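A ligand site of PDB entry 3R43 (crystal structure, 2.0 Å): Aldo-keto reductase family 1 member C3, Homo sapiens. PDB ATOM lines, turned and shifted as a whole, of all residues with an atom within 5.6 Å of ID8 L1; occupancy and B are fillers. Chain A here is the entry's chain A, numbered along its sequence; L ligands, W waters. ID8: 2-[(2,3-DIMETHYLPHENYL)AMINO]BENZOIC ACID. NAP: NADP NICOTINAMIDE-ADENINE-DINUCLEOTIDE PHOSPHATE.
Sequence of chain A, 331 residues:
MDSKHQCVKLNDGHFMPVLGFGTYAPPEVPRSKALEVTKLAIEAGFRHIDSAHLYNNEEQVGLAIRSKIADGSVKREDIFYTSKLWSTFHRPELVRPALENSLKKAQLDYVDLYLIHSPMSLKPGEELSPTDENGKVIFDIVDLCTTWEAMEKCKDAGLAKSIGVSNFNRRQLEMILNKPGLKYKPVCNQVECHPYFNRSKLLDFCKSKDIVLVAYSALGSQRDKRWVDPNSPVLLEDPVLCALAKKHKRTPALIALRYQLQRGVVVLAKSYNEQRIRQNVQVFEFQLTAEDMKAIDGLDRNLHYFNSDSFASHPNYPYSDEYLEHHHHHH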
ATOM      1  N   TYR A  24     -18.773  33.297  -4.404  1.00  0.00           N
ATOM      2  CA  TYR A  24     -17.663  32.482  -3.955  1.00  0.00           C
ATOM      3  C   TYR A  24     -16.380  32.811  -4.782  1.00  0.00           C
ATOM      4  O   TYR A  24     -16.425  32.881  -6.002  1.00  0.00           O
ATOM      5  CB  TYR A  24     -17.924  30.984  -4.053  1.00  0.00           C
ATOM      6  CG  TYR A  24     -16.694  30.218  -3.618  1.00  0.00           C
ATOM      7  CD1 TYR A  24     -16.353  30.125  -2.250  1.00  0.00           C
ATOM      8  CD2 TYR A  24     -15.848  29.590  -4.566  1.00  0.00           C
ATOM      9  CE1 TYR A  24     -15.236  29.423  -1.815  1.00  0.00           C
ATOM     10  CE2 TYR A  24     -14.688  28.905  -4.139  1.00  0.00           C
ATOM     11  CZ  TYR A  24     -14.405  28.831  -2.743  1.00  0.00           C
ATOM     12  OH  TYR A  24     -13.324  28.148  -2.277  1.00  0.00           O
ATOM     13  N   ALA A  52     -22.606  32.419   1.695  1.00  0.00           N
ATOM     14  CA  ALA A  52     -22.684  31.234   2.534  1.00  0.00           C
ATOM     15  C   ALA A  52     -21.619  31.341   3.620  1.00  0.00           C
ATOM     16  O   ALA A  52     -20.602  32.021   3.440  1.00  0.00           O
ATOM     17  CB  ALA A  52     -22.472  29.894   1.713  1.00  0.00           C
ATOM     18  N   LEU A  54     -19.719  28.961   4.338  1.00  0.00           N
ATOM     19  CA  LEU A  54     -18.558  28.323   3.675  1.00  0.00           C
ATOM     20  C   LEU A  54     -17.603  29.334   3.004  1.00  0.00           C
ATOM     21  O   LEU A  54     -16.384  29.113   2.956  1.00  0.00           O
ATOM     22  CB  LEU A  54     -18.988  27.309   2.633  1.00  0.00           C
ATOM     23  CG  LEU A  54     -17.880  26.437   2.009  1.00  0.00           C
ATOM     24  CD1 LEU A  54     -17.132  25.517   3.059  1.00  0.00           C
ATOM     25  CD2 LEU A  54     -18.451  25.598   0.837  1.00  0.00           C
ATOM     26  N   TYR A  55     -18.157  30.422   2.458  1.00  0.00           N
ATOM     27  CA  TYR A  55     -17.389  31.281   1.537  1.00  0.00           C
ATOM     28  C   TYR A  55     -16.419  32.251   2.220  1.00  0.00           C
ATOM     29  O   TYR A  55     -15.489  32.772   1.571  1.00  0.00           O
ATOM     30  CB  TYR A  55     -18.281  32.069   0.574  1.00  0.00           C
ATOM     31  CG  TYR A  55     -19.272  31.203  -0.206  1.00  0.00           C
ATOM     32  CD1 TYR A  55     -19.086  29.824  -0.304  1.00  0.00           C
ATOM     33  CD2 TYR A  55     -20.362  31.787  -0.879  1.00  0.00           C
ATOM     34  CE1 TYR A  55     -20.002  29.010  -1.020  1.00  0.00           C
ATOM     35  CE2 TYR A  55     -21.260  31.004  -1.603  1.00  0.00           C
ATOM     36  CZ  TYR A  55     -21.095  29.630  -1.660  1.00  0.00           C
ATOM     37  OH  TYR A  55     -21.987  28.837  -2.343  1.00  0.00           O
ATOM     38  N   LYS A  84     -26.191  30.348   3.762  1.00  0.00           N
ATOM     39  CA  LYS A  84     -26.388  28.904   3.792  1.00  0.00           C
ATOM     40  C   LYS A  84     -25.733  28.329   5.016  1.00  0.00           C
ATOM     41  O   LYS A  84     -24.603  28.686   5.383  1.00  0.00           O
ATOM     42  CB  LYS A  84     -25.773  28.231   2.578  1.00  0.00           C
ATOM     43  CG  LYS A  84     -26.209  28.826   1.200  1.00  0.00           C
ATOM     44  CD  LYS A  84     -25.563  28.005   0.083  1.00  0.00           C
ATOM     45  CE  LYS A  84     -25.799  28.690  -1.279  1.00  0.00           C
ATOM     46  NZ  LYS A  84     -24.742  29.704  -1.510  1.00  0.00           N
ATOM     47  N   TRP A  86     -23.830  25.826   7.015  1.00  0.00           N
ATOM     48  CA  TRP A  86     -22.799  24.821   6.728  1.00  0.00           C
ATOM     49  C   TRP A  86     -23.059  23.434   7.366  1.00  0.00           C
ATOM     50  O   TRP A  86     -23.828  23.304   8.340  1.00  0.00           O
ATOM     51  CB  TRP A  86     -21.368  25.423   6.915  1.00  0.00           C
ATOM     52  CG  TRP A  86     -20.350  24.395   6.446  1.00  0.00           C
ATOM     53  CD1 TRP A  86     -19.405  23.738   7.216  1.00  0.00           C
ATOM     54  CD2 TRP A  86     -20.284  23.807   5.152  1.00  0.00           C
ATOM     55  NE1 TRP A  86     -18.724  22.821   6.459  1.00  0.00           N
ATOM     56  CE2 TRP A  86     -19.252  22.829   5.186  1.00  0.00           C
ATOM     57  CE3 TRP A  86     -20.978  24.029   3.940  1.00  0.00           C
ATOM     58  CZ2 TRP A  86     -18.895  22.066   4.053  1.00  0.00           C
ATOM     59  CZ3 TRP A  86     -20.627  23.234   2.805  1.00  0.00           C
ATOM     60  CH2 TRP A  86     -19.613  22.286   2.878  1.00  0.00           C
ATOM     61  N   SER A  87     -22.417  22.390   6.827  1.00  0.00           N
ATOM     62  CA  SER A  87     -22.773  20.991   7.066  1.00  0.00           C
ATOM     63  C   SER A  87     -22.283  20.451   8.419  1.00  0.00           C
ATOM     64  O   SER A  87     -22.650  19.340   8.851  1.00  0.00           O
ATOM     65  CB  SER A  87     -22.221  20.106   5.908  1.00  0.00           C
ATOM     66  OG  SER A  87     -22.648  20.637   4.661  1.00  0.00           O
ATOM     67  N   HIS A 117     -26.896  23.955   3.043  1.00  0.00           N
ATOM     68  CA  HIS A 117     -25.924  24.057   1.959  1.00  0.00           C
ATOM     69  C   HIS A 117     -25.807  22.713   1.268  1.00  0.00           C
ATOM     70  O   HIS A 117     -25.581  22.653   0.025  1.00  0.00           O
ATOM     71  CB  HIS A 117     -24.534  24.490   2.489  1.00  0.00           C
ATOM     72  CG  HIS A 117     -23.636  25.111   1.470  1.00  0.00           C
ATOM     73  ND1 HIS A 117     -22.798  26.169   1.770  1.00  0.00           N
ATOM     74  CD2 HIS A 117     -23.392  24.797   0.166  1.00  0.00           C
ATOM     75  CE1 HIS A 117     -22.091  26.493   0.688  1.00  0.00           C
ATOM     76  NE2 HIS A 117     -22.416  25.663  -0.292  1.00  0.00           N
ATOM     77  N   SER A 118     -25.891  21.639   2.058  1.00  0.00           N
ATOM     78  CA  SER A 118     -25.632  20.324   1.480  1.00  0.00           C
ATOM     79  C   SER A 118     -26.335  19.294   2.345  1.00  0.00           C
ATOM     80  O   SER A 118     -26.493  19.536   3.535  1.00  0.00           O
ATOM     81  CB  SER A 118     -24.105  20.097   1.416  1.00  0.00           C
ATOM     82  OG  SER A 118     -23.758  18.740   1.368  1.00  0.00           O
ATOM     83  N   MET A 120     -24.963  16.506   3.014  1.00  0.00           N
ATOM     84  CA  MET A 120     -23.904  15.641   3.500  1.00  0.00           C
ATOM     85  C   MET A 120     -23.330  16.123   4.831  1.00  0.00           C
ATOM     86  O   MET A 120     -22.356  16.891   4.865  1.00  0.00           O
ATOM     87  CB  MET A 120     -22.784  15.498   2.448  1.00  0.00           C
ATOM     88  CG  MET A 120     -23.275  14.738   1.137  1.00  0.00           C
ATOM     89  SD  MET A 120     -21.982  14.775  -0.120  1.00  0.00           S
ATOM     90  CE  MET A 120     -22.052  16.515  -0.585  1.00  0.00           C
ATOM     91  N   ASN A 167     -28.200  21.278  -3.089  1.00  0.00           N
ATOM     92  CA  ASN A 167     -27.544  19.977  -3.347  1.00  0.00           C
ATOM     93  C   ASN A 167     -28.346  18.726  -2.963  1.00  0.00           C
ATOM     94  O   ASN A 167     -27.756  17.639  -2.710  1.00  0.00           O
ATOM     95  CB  ASN A 167     -26.164  19.926  -2.714  1.00  0.00           C
ATOM     96  CG  ASN A 167     -25.203  20.865  -3.398  1.00  0.00           C
ATOM     97  OD1 ASN A 167     -25.004  20.797  -4.617  1.00  0.00           O
ATOM     98  ND2 ASN A 167     -24.599  21.779  -2.624  1.00  0.00           N
ATOM     99  N   TYR A 216     -26.392  26.651  -9.932  1.00  0.00           N
ATOM    100  CA  TYR A 216     -25.035  27.124  -9.750  1.00  0.00           C
ATOM    101  C   TYR A 216     -24.092  26.403 -10.721  1.00  0.00           C
ATOM    102  O   TYR A 216     -24.484  25.400 -11.343  1.00  0.00           O
ATOM    103  CB  TYR A 216     -24.563  26.959  -8.305  1.00  0.00           C
ATOM    104  CG  TYR A 216     -24.255  25.519  -7.819  1.00  0.00           C
ATOM    105  CD1 TYR A 216     -23.169  24.812  -8.317  1.00  0.00           C
ATOM    106  CD2 TYR A 216     -25.064  24.891  -6.839  1.00  0.00           C
ATOM    107  CE1 TYR A 216     -22.859  23.558  -7.810  1.00  0.00           C
ATOM    108  CE2 TYR A 216     -24.779  23.634  -6.349  1.00  0.00           C
ATOM    109  CZ  TYR A 216     -23.683  22.985  -6.825  1.00  0.00           C
ATOM    110  OH  TYR A 216     -23.393  21.736  -6.386  1.00  0.00           O
ATOM    111  N   TRP A 227     -11.735  20.186  -6.480  1.00  0.00           N
ATOM    112  CA  TRP A 227     -12.926  19.316  -6.700  1.00  0.00           C
ATOM    113  C   TRP A 227     -13.203  19.034  -8.162  1.00  0.00           C
ATOM    114  O   TRP A 227     -14.018  18.159  -8.459  1.00  0.00           O
ATOM    115  CB  TRP A 227     -14.226  19.849  -6.014  1.00  0.00           C
ATOM    116  CG  TRP A 227     -13.970  20.277  -4.604  1.00  0.00           C
ATOM    117  CD1 TRP A 227     -13.860  19.468  -3.492  1.00  0.00           C
ATOM    118  CD2 TRP A 227     -13.668  21.588  -4.196  1.00  0.00           C
ATOM    119  NE1 TRP A 227     -13.522  20.241  -2.378  1.00  0.00           N
ATOM    120  CE2 TRP A 227     -13.393  21.540  -2.793  1.00  0.00           C
ATOM    121  CE3 TRP A 227     -13.624  22.815  -4.867  1.00  0.00           C
ATOM    122  CZ2 TRP A 227     -13.112  22.675  -2.051  1.00  0.00           C
ATOM    123  CZ3 TRP A 227     -13.315  23.938  -4.134  1.00  0.00           C
ATOM    124  CH2 TRP A 227     -13.056  23.863  -2.733  1.00  0.00           C
ATOM    125  N   PHE A 306     -18.200  19.198 -10.000  1.00  0.00           N
ATOM    126  CA  PHE A 306     -17.736  18.917  -8.617  1.00  0.00           C
ATOM    127  C   PHE A 306     -17.739  17.409  -8.495  1.00  0.00           C
ATOM    128  O   PHE A 306     -18.807  16.801  -8.494  1.00  0.00           O
ATOM    129  CB  PHE A 306     -18.683  19.550  -7.580  1.00  0.00           C
ATOM    130  CG  PHE A 306     -18.481  21.045  -7.430  1.00  0.00           C
ATOM    131  CD1 PHE A 306     -17.629  21.547  -6.489  1.00  0.00           C
ATOM    132  CD2 PHE A 306     -19.140  21.942  -8.266  1.00  0.00           C
ATOM    133  CE1 PHE A 306     -17.425  22.924  -6.325  1.00  0.00           C
ATOM    134  CE2 PHE A 306     -18.940  23.333  -8.130  1.00  0.00           C
ATOM    135  CZ  PHE A 306     -18.085  23.820  -7.161  1.00  0.00           C
ATOM    136  N   PHE A 311     -16.979  14.098  -1.582  1.00  0.00           N
ATOM    137  CA  PHE A 311     -18.417  14.012  -1.649  1.00  0.00           C
ATOM    138  C   PHE A 311     -18.846  12.600  -1.945  1.00  0.00           C
ATOM    139  O   PHE A 311     -19.795  12.129  -1.304  1.00  0.00           O
ATOM    140  CB  PHE A 311     -19.033  14.963  -2.716  1.00  0.00           C
ATOM    141  CG  PHE A 311     -18.472  16.362  -2.689  1.00  0.00           C
ATOM    142  CD1 PHE A 311     -18.497  17.122  -1.501  1.00  0.00           C
ATOM    143  CD2 PHE A 311     -17.932  16.938  -3.848  1.00  0.00           C
ATOM    144  CE1 PHE A 311     -17.958  18.420  -1.469  1.00  0.00           C
ATOM    145  CE2 PHE A 311     -17.392  18.258  -3.840  1.00  0.00           C
ATOM    146  CZ  PHE A 311     -17.406  18.998  -2.647  1.00  0.00           C
ATOM    147  N   PRO A 318     -25.540  13.288  -2.910  1.00  0.00           N
ATOM    148  CA  PRO A 318     -26.739  13.475  -3.686  1.00  0.00           C
ATOM    149  C   PRO A 318     -26.705  12.808  -5.066  1.00  0.00           C
ATOM    150  O   PRO A 318     -27.772  12.521  -5.611  1.00  0.00           O
ATOM    151  CB  PRO A 318     -26.869  15.011  -3.813  1.00  0.00           C
ATOM    152  CG  PRO A 318     -25.543  15.467  -3.772  1.00  0.00           C
ATOM    153  CD  PRO A 318     -24.755  14.534  -2.825  1.00  0.00           C
ATOM    154  N   TYR A 319     -25.521  12.499  -5.613  1.00  0.00           N
ATOM    155  CA  TYR A 319     -25.523  11.994  -6.977  1.00  0.00           C
ATOM    156  C   TYR A 319     -25.601  10.453  -7.043  1.00  0.00           C
ATOM    157  O   TYR A 319     -25.512   9.868  -8.127  1.00  0.00           O
ATOM    158  CB  TYR A 319     -24.386  12.550  -7.853  1.00  0.00           C
ATOM    159  CG  TYR A 319     -24.326  14.078  -7.870  1.00  0.00           C
ATOM    160  CD1 TYR A 319     -25.457  14.838  -8.170  1.00  0.00           C
ATOM    161  CD2 TYR A 319     -23.137  14.741  -7.624  1.00  0.00           C
ATOM    162  CE1 TYR A 319     -25.413  16.256  -8.227  1.00  0.00           C
ATOM    163  CE2 TYR A 319     -23.093  16.159  -7.682  1.00  0.00           C
ATOM    164  CZ  TYR A 319     -24.253  16.888  -7.987  1.00  0.00           C
ATOM    165  OH  TYR A 319     -24.227  18.273  -8.027  1.00  0.00           O
HETATM  166  O16 ID8 L   1     -20.917  26.604  -2.501  1.00  0.00           O
HETATM  167  C14 ID8 L   1     -19.940  26.717  -3.258  1.00  0.00           C
HETATM  168  O15 ID8 L   1     -19.763  27.713  -3.992  1.00  0.00           O
HETATM  169  C13 ID8 L   1     -18.773  25.757  -3.052  1.00  0.00           C
HETATM  170  C12 ID8 L   1     -17.493  26.312  -3.254  1.00  0.00           C
HETATM  171  C11 ID8 L   1     -16.352  25.467  -3.078  1.00  0.00           C
HETATM  172  C10 ID8 L   1     -16.535  24.111  -2.715  1.00  0.00           C
HETATM  173  C9  ID8 L   1     -17.810  23.565  -2.509  1.00  0.00           C
HETATM  174  C8  ID8 L   1     -18.946  24.399  -2.666  1.00  0.00           C
HETATM  175  N7  ID8 L   1     -20.182  23.881  -2.517  1.00  0.00           N
HETATM  176  C6  ID8 L   1     -20.522  22.614  -2.155  1.00  0.00           C
HETATM  177  C1  ID8 L   1     -20.751  21.589  -3.097  1.00  0.00           C
HETATM  178  C17 ID8 L   1     -20.527  21.827  -4.615  1.00  0.00           C
HETATM  179  C5  ID8 L   1     -20.712  22.314  -0.790  1.00  0.00           C
HETATM  180  C4  ID8 L   1     -21.092  21.037  -0.354  1.00  0.00           C
HETATM  181  C3  ID8 L   1     -21.289  20.009  -1.300  1.00  0.00           C
HETATM  182  C2  ID8 L   1     -21.129  20.296  -2.654  1.00  0.00           C
HETATM  183  C18 ID8 L   1     -21.358  19.129  -3.665  1.00  0.00           C
HETATM  184  PA  NAP L   2     -19.973  30.174 -12.385  1.00  0.00           P
HETATM  185  O1A NAP L   2     -21.144  31.050 -12.266  1.00  0.00           O
HETATM  186  O2A NAP L   2     -20.195  28.819 -13.039  1.00  0.00           O
HETATM  187  O5B NAP L   2     -18.731  30.837 -13.192  1.00  0.00           O
HETATM  188  C5B NAP L   2     -17.515  30.159 -13.589  1.00  0.00           C
HETATM  189  C4B NAP L   2     -16.520  31.180 -14.195  1.00  0.00           C
HETATM  190  O4B NAP L   2     -17.265  31.821 -15.232  1.00  0.00           O
HETATM  191  C3B NAP L   2     -16.336  32.329 -13.199  1.00  0.00           C
HETATM  192  O3B NAP L   2     -15.202  32.028 -12.389  1.00  0.00           O
HETATM  193  C2B NAP L   2     -16.124  33.547 -14.087  1.00  0.00           C
HETATM  194  O2B NAP L   2     -14.737  33.905 -14.206  1.00  0.00           O
HETATM  195  C1B NAP L   2     -16.558  33.049 -15.449  1.00  0.00           C
HETATM  196  N9A NAP L   2     -17.471  34.026 -16.093  1.00  0.00           N
HETATM  197  C8A NAP L   2     -18.475  34.675 -15.513  1.00  0.00           C
HETATM  198  N7A NAP L   2     -19.060  35.418 -16.430  1.00  0.00           N
HETATM  199  C5A NAP L   2     -18.478  35.196 -17.594  1.00  0.00           C
HETATM  200  C6A NAP L   2     -18.642  35.724 -18.887  1.00  0.00           C
HETATM  201  N6A NAP L   2     -19.620  36.612 -19.145  1.00  0.00           N
HETATM  202  N1A NAP L   2     -17.811  35.313 -19.861  1.00  0.00           N
HETATM  203  C2A NAP L   2     -16.830  34.410 -19.629  1.00  0.00           C
HETATM  204  N3A NAP L   2     -16.646  33.915 -18.407  1.00  0.00           N
HETATM  205  C4A NAP L   2     -17.447  34.298 -17.382  1.00  0.00           C
HETATM  206  O3  NAP L   2     -19.248  29.805 -11.023  1.00  0.00           O
HETATM  207  PN  NAP L   2     -19.604  29.047  -9.664  1.00  0.00           P
HETATM  208  O1N NAP L   2     -18.751  29.775  -8.678  1.00  0.00           O
HETATM  209  O2N NAP L   2     -19.455  27.583  -9.831  1.00  0.00           O
HETATM  210  O5D NAP L   2     -21.182  29.327  -9.463  1.00  0.00           O
HETATM  211  C5D NAP L   2     -21.809  30.579  -9.162  1.00  0.00           C
HETATM  212  C4D NAP L   2     -22.188  30.717  -7.708  1.00  0.00           C
HETATM  213  O4D NAP L   2     -23.147  29.696  -7.310  1.00  0.00           O
HETATM  214  C3D NAP L   2     -20.999  30.595  -6.708  1.00  0.00           C
HETATM  215  O3D NAP L   2     -20.193  31.838  -6.642  1.00  0.00           O
HETATM  216  C2D NAP L   2     -21.796  30.419  -5.432  1.00  0.00           C
HETATM  217  O2D NAP L   2     -22.393  31.685  -5.088  1.00  0.00           O
HETATM  218  C1D NAP L   2     -22.959  29.475  -5.908  1.00  0.00           C
HETATM  219  N1N NAP L   2     -22.511  28.055  -5.806  1.00  0.00           N
HETATM  220  C2N NAP L   2     -23.162  27.300  -4.849  1.00  0.00           C
HETATM  221  C3N NAP L   2     -22.823  25.952  -4.691  1.00  0.00           C
HETATM  222  C7N NAP L   2     -23.555  25.117  -3.648  1.00  0.00           C
HETATM  223  O7N NAP L   2     -23.002  24.129  -3.186  1.00  0.00           O
HETATM  224  N7N NAP L   2     -24.840  25.488  -3.358  1.00  0.00           N
HETATM  225  C4N NAP L   2     -21.779  25.412  -5.452  1.00  0.00           C
HETATM  226  C5N NAP L   2     -21.122  26.177  -6.437  1.00  0.00           C
HETATM  227  C6N NAP L   2     -21.465  27.518  -6.630  1.00  0.00           C
HETATM  228  P2B NAP L   2     -14.358  35.454 -13.713  1.00  0.00           P
HETATM  229  O1X NAP L   2     -14.568  35.647 -12.238  1.00  0.00           O
HETATM  230  O2X NAP L   2     -12.883  35.579 -14.162  1.00  0.00           O
HETATM  231  O3X NAP L   2     -15.219  36.379 -14.633  1.00  0.00           O
HETATM  232  O   HOH W   1     -18.085  27.791  -6.286  1.00  0.00           O
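N7 of ID8 L1 sits at hydrogen-bond distance from O7N of NAP L2, 2.9 Å away.
The side-chain amino group of Lys 84 lies within hydrogen-bond range of the side-chain hydroxyl of Tyr 55, at 3.0 Å.
O of His 117 is in hydrogen-bond range of ND2 of Asn 167 (3.0 Å).
The side-chain hydroxyl (OH) of Tyr 216 lies within hydrogen-bond range of the side-chain amide oxygen (OD1) of Asn 167 (2.6 Å).
OG of Ser 118 sits at hydrogen-bond distance from N of Met 120 (3.0 Å).
An oxygen (O16) of ID8 L1 sits at hydrogen-bond distance from the side-chain hydroxyl (OH) of Tyr 55, at 2.5 Å.
An oxygen (O16) of ID8 L1 sits at hydrogen-bond distance from a ring nitrogen (NE2) of His 117, 2.8 Å away.
O7N of NAP L2 sits at hydrogen-bond distance from NE2 of His 117, at 3.3 Å.
The backbone NH of Tyr 24 lies within hydrogen-bond range of an oxygen (O3D) of NAP L2 (3.0 Å).
O7N of NAP L2 sits at hydrogen-bond distance from ND2 of Asn 167.
Water W1 lies within hydrogen-bond range of O15 of ID8 L1 (2.8 Å) and O1N of NAP L2 (3.2 Å).
Tyr 24 touches ID8 L1.
Leu 54 touches ID8 L1.
Trp 86 touches ID8 L1 (CZ3 to C5, 3.7 Å).
CB of Ser 118 touches C4 of ID8 L1, 3.6 Å away.
CE of Met 120 touches C3 of ID8 L1, at 3.6 Å.
ND2 of Asn 167 touches C2 of ID8 L1 (3.8 Å).
OH of Tyr 216 touches C17 of ID8 L1, at 3.4 Å.
CH2 of Trp 227 touches C10 of ID8 L1, at 3.5 Å.
Phe 306 touches ID8 L1.
CE1 of Phe 311 touches C3 of ID8 L1 (3.7 Å).
Hydrophobic or aromatic side chains within 4 Å of ID8 L1: Tyr 24, Leu 54, Tyr 55, Trp 86, His 117, Met 120, Trp 227, Phe 306 and Phe 311.
12 residues have an atom within 4 Å of ID8 L1: Tyr 24, Leu 54, Tyr 55, Trp 86, His 117, Ser 118, Met 120, Asn 167, Tyr 216, Trp 227, Phe 306 and Phe 311.
The nearest printed residue that does not touch ID8 L1 is Lys 84 (5.0 Å).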
